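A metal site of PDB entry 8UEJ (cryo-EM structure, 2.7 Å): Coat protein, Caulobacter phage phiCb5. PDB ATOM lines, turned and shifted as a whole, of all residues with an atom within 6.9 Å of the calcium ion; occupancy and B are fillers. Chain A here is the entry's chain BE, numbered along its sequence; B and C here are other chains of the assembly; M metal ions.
The calcium ion is bound by O of Gln 25 of chain A (2.3 Å). The backbone carbonyl oxygen (O) of Gln 25 of chain B is bound to the calcium ion. O of Gln 25 of chain C binds the calcium ion (2.5 Å). OD1 of Asp 26 of chain A binds the calcium ion (2.8 Å). The calcium ion has four donor atoms within binding distance. Slightly farther from the calcium ion lies OD1 of Asp 26 of chain C (3.1 Å).
The side-chain amide oxygen of Asn 24 of chain B sits close to the side-chain carboxylate of Asp 26 of chain B (2.9 Å). The side-chain carboxylate of Asp 26 of chain C sits at hydrogen-bond distance from the backbone NH of Gly 27 of chain A, at 3.1 Å. The side-chain amide oxygen of Asn 24 of chain C lies within hydrogen-bond range of the side-chain amide nitrogen of Gln 25 of chain A (2.7 Å). O of Asp 26 of chain B is in hydrogen-bond range of ND2 of Asn 24 of chain A (2.6 Å). The backbone NH (N) of Gly 27 of chain C sits at hydrogen-bond distance from the side-chain carboxylate (OD2) of Asp 26 of chain B, at 3.3 Å. The side-chain amide oxygen (OD1) of Asn 24 of chain B lies close to the side-chain amide oxygen (OE1) of Gln 25 of chain C (3.1 Å). The side-chain carboxylate (OD2) of Asp 26 of chain A sits close to the backbone carbonyl oxygen (O) of Asp 26 of chain B, 2.5 Å away.
Residues that only touch the calcium ion: Asp 26 of chain B. Of the 13 residues printed, 6 come within 4 Å of the calcium ion. Along chain A the residues within 4 Å of the calcium ion span positions 25 to 26. The nearest printed residue that does not touch the calcium ion is Asn 24 of chain B (4.6 Å).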
ATOM      1  N   ASN A  24      -6.317  -9.270  -8.183  1.00  0.00           N
ATOM      2  CA  ASN A  24      -7.318 -10.242  -7.770  1.00  0.00           C
ATOM      3  C   ASN A  24      -8.557 -10.047  -8.632  1.00  0.00           C
ATOM      4  O   ASN A  24      -8.750  -8.987  -9.244  1.00  0.00           O
ATOM      5  CB  ASN A  24      -7.668 -10.090  -6.282  1.00  0.00           C
ATOM      6  CG  ASN A  24      -8.473 -11.259  -5.756  1.00  0.00           C
ATOM      7  OD1 ASN A  24      -9.452 -11.074  -5.044  1.00  0.00           O
ATOM      8  ND2 ASN A  24      -8.036 -12.477  -6.081  1.00  0.00           N
ATOM      9  N   GLN A  25      -9.390 -11.091  -8.693  1.00  0.00           N
ATOM     10  CA  GLN A  25     -10.652 -11.013  -9.435  1.00  0.00           C
ATOM     11  C   GLN A  25     -11.561 -12.121  -8.897  1.00  0.00           C
ATOM     12  O   GLN A  25     -11.363 -13.290  -9.235  1.00  0.00           O
ATOM     13  CB  GLN A  25     -10.414 -11.163 -10.928  1.00  0.00           C
ATOM     14  CG  GLN A  25     -11.624 -10.794 -11.757  1.00  0.00           C
ATOM     15  CD  GLN A  25     -12.618 -11.926 -11.906  1.00  0.00           C
ATOM     16  OE1 GLN A  25     -12.230 -13.085 -12.029  1.00  0.00           O
ATOM     17  NE2 GLN A  25     -13.893 -11.586 -11.832  1.00  0.00           N
ATOM     18  N   ASP A  26     -12.540 -11.740  -8.080  1.00  0.00           N
ATOM     19  CA  ASP A  26     -13.469 -12.708  -7.508  1.00  0.00           C
ATOM     20  C   ASP A  26     -14.869 -12.121  -7.429  1.00  0.00           C
ATOM     21  O   ASP A  26     -15.034 -10.917  -7.205  1.00  0.00           O
ATOM     22  CB  ASP A  26     -13.027 -13.149  -6.108  1.00  0.00           C
ATOM     23  CG  ASP A  26     -11.963 -14.228  -6.124  1.00  0.00           C
ATOM     24  OD1 ASP A  26     -11.751 -14.839  -7.198  1.00  0.00           O
ATOM     25  OD2 ASP A  26     -11.349 -14.470  -5.074  1.00  0.00           O
ATOM     26  N   GLY A  27     -15.859 -12.977  -7.605  1.00  0.00           N
ATOM     27  CA  GLY A  27     -17.237 -12.572  -7.375  1.00  0.00           C
ATOM     28  C   GLY A  27     -17.675 -11.374  -8.194  1.00  0.00           C
ATOM     29  O   GLY A  27     -18.276 -10.441  -7.655  1.00  0.00           O
ATOM     30  N   ASN B  24      -6.740 -21.298 -12.324  1.00  0.00           N
ATOM     31  CA  ASN B  24      -7.553 -20.652 -11.302  1.00  0.00           C
ATOM     32  C   ASN B  24      -6.717 -19.626 -10.540  1.00  0.00           C
ATOM     33  O   ASN B  24      -5.489 -19.695 -10.515  1.00  0.00           O
ATOM     34  CB  ASN B  24      -8.138 -21.671 -10.320  1.00  0.00           C
ATOM     35  CG  ASN B  24      -9.119 -21.045  -9.350  1.00  0.00           C
ATOM     36  OD1 ASN B  24      -9.372 -19.849  -9.390  1.00  0.00           O
ATOM     37  ND2 ASN B  24      -9.669 -21.866  -8.451  1.00  0.00           N
ATOM     38  N   GLN B  25      -7.415 -18.672  -9.929  1.00  0.00           N
ATOM     39  CA  GLN B  25      -6.808 -17.779  -8.945  1.00  0.00           C
ATOM     40  C   GLN B  25      -7.923 -17.056  -8.202  1.00  0.00           C
ATOM     41  O   GLN B  25      -8.669 -16.289  -8.808  1.00  0.00           O
ATOM     42  CB  GLN B  25      -5.858 -16.785  -9.615  1.00  0.00           C
ATOM     43  CG  GLN B  25      -6.522 -15.802 -10.558  1.00  0.00           C
ATOM     44  CD  GLN B  25      -5.530 -14.881 -11.248  1.00  0.00           C
ATOM     45  OE1 GLN B  25      -4.328 -14.939 -10.977  1.00  0.00           O
ATOM     46  NE2 GLN B  25      -6.031 -14.020 -12.125  1.00  0.00           N
ATOM     47  N   ASP B  26      -8.048 -17.316  -6.888  1.00  0.00           N
ATOM     48  CA  ASP B  26      -9.092 -16.692  -6.086  1.00  0.00           C
ATOM     49  C   ASP B  26      -8.545 -15.837  -4.955  1.00  0.00           C
ATOM     50  O   ASP B  26      -8.851 -14.638  -4.889  1.00  0.00           O
ATOM     51  CB  ASP B  26     -10.031 -17.771  -5.540  1.00  0.00           C
ATOM     52  CG  ASP B  26     -10.686 -18.585  -6.638  1.00  0.00           C
ATOM     53  OD1 ASP B  26     -10.917 -18.033  -7.736  1.00  0.00           O
ATOM     54  OD2 ASP B  26     -10.963 -19.791  -6.414  1.00  0.00           O
ATOM     55  N   GLY B  27      -7.733 -16.402  -4.068  1.00  0.00           N
ATOM     56  CA  GLY B  27      -7.306 -15.671  -2.883  1.00  0.00           C
ATOM     57  C   GLY B  27      -5.940 -15.027  -3.039  1.00  0.00           C
ATOM     58  O   GLY B  27      -5.033 -15.280  -2.240  1.00  0.00           O
ATOM     59  N   THR B  29      -3.876 -15.830  -5.045  1.00  0.00           N
ATOM     60  CA  THR B  29      -2.991 -16.920  -5.415  1.00  0.00           C
ATOM     61  C   THR B  29      -3.444 -17.474  -6.758  1.00  0.00           C
ATOM     62  O   THR B  29      -4.640 -17.489  -7.055  1.00  0.00           O
ATOM     63  CB  THR B  29      -3.004 -18.046  -4.373  1.00  0.00           C
ATOM     64  OG1 THR B  29      -4.260 -18.730  -4.431  1.00  0.00           O
ATOM     65  CG2 THR B  29      -2.792 -17.502  -2.987  1.00  0.00           C
ATOM     66  N   ASN C  24     -15.787 -13.585 -15.036  1.00  0.00           N
ATOM     67  CA  ASN C  24     -15.454 -14.184 -13.752  1.00  0.00           C
ATOM     68  C   ASN C  24     -14.645 -15.451 -13.972  1.00  0.00           C
ATOM     69  O   ASN C  24     -14.683 -16.046 -15.050  1.00  0.00           O
ATOM     70  CB  ASN C  24     -16.728 -14.508 -12.959  1.00  0.00           C
ATOM     71  CG  ASN C  24     -16.592 -14.183 -11.491  1.00  0.00           C
ATOM     72  OD1 ASN C  24     -15.673 -13.489 -11.079  1.00  0.00           O
ATOM     73  ND2 ASN C  24     -17.521 -14.695 -10.688  1.00  0.00           N
ATOM     74  N   GLN C  25     -13.886 -15.834 -12.947  1.00  0.00           N
ATOM     75  CA  GLN C  25     -13.279 -17.168 -12.903  1.00  0.00           C
ATOM     76  C   GLN C  25     -13.049 -17.515 -11.438  1.00  0.00           C
ATOM     77  O   GLN C  25     -12.101 -17.021 -10.819  1.00  0.00           O
ATOM     78  CB  GLN C  25     -11.977 -17.217 -13.689  1.00  0.00           C
ATOM     79  CG  GLN C  25     -11.447 -18.631 -13.822  1.00  0.00           C
ATOM     80  CD  GLN C  25     -10.614 -19.072 -12.657  1.00  0.00           C
ATOM     81  OE1 GLN C  25      -9.956 -18.265 -12.001  1.00  0.00           O
ATOM     82  NE2 GLN C  25     -10.674 -20.363 -12.346  1.00  0.00           N
ATOM     83  N   ASP C  26     -13.911 -18.373 -10.888  1.00  0.00           N
ATOM     84  CA  ASP C  26     -13.824 -18.800  -9.499  1.00  0.00           C
ATOM     85  C   ASP C  26     -14.003 -20.316  -9.415  1.00  0.00           C
ATOM     86  O   ASP C  26     -14.821 -20.893 -10.132  1.00  0.00           O
ATOM     87  CB  ASP C  26     -14.884 -18.120  -8.632  1.00  0.00           C
ATOM     88  CG  ASP C  26     -14.579 -16.656  -8.375  1.00  0.00           C
ATOM     89  OD1 ASP C  26     -13.541 -16.166  -8.869  1.00  0.00           O
ATOM     90  OD2 ASP C  26     -15.375 -16.003  -7.667  1.00  0.00           O
ATOM     91  N   GLY C  27     -13.247 -20.940  -8.513  1.00  0.00           N
ATOM     92  CA  GLY C  27     -13.408 -22.349  -8.224  1.00  0.00           C
ATOM     93  C   GLY C  27     -13.277 -23.246  -9.437  1.00  0.00           C
ATOM     94  O   GLY C  27     -14.056 -24.178  -9.618  1.00  0.00           O
HETATM   95 CA    CA M   1     -10.624 -15.398  -9.694  1.00  0.00          CA
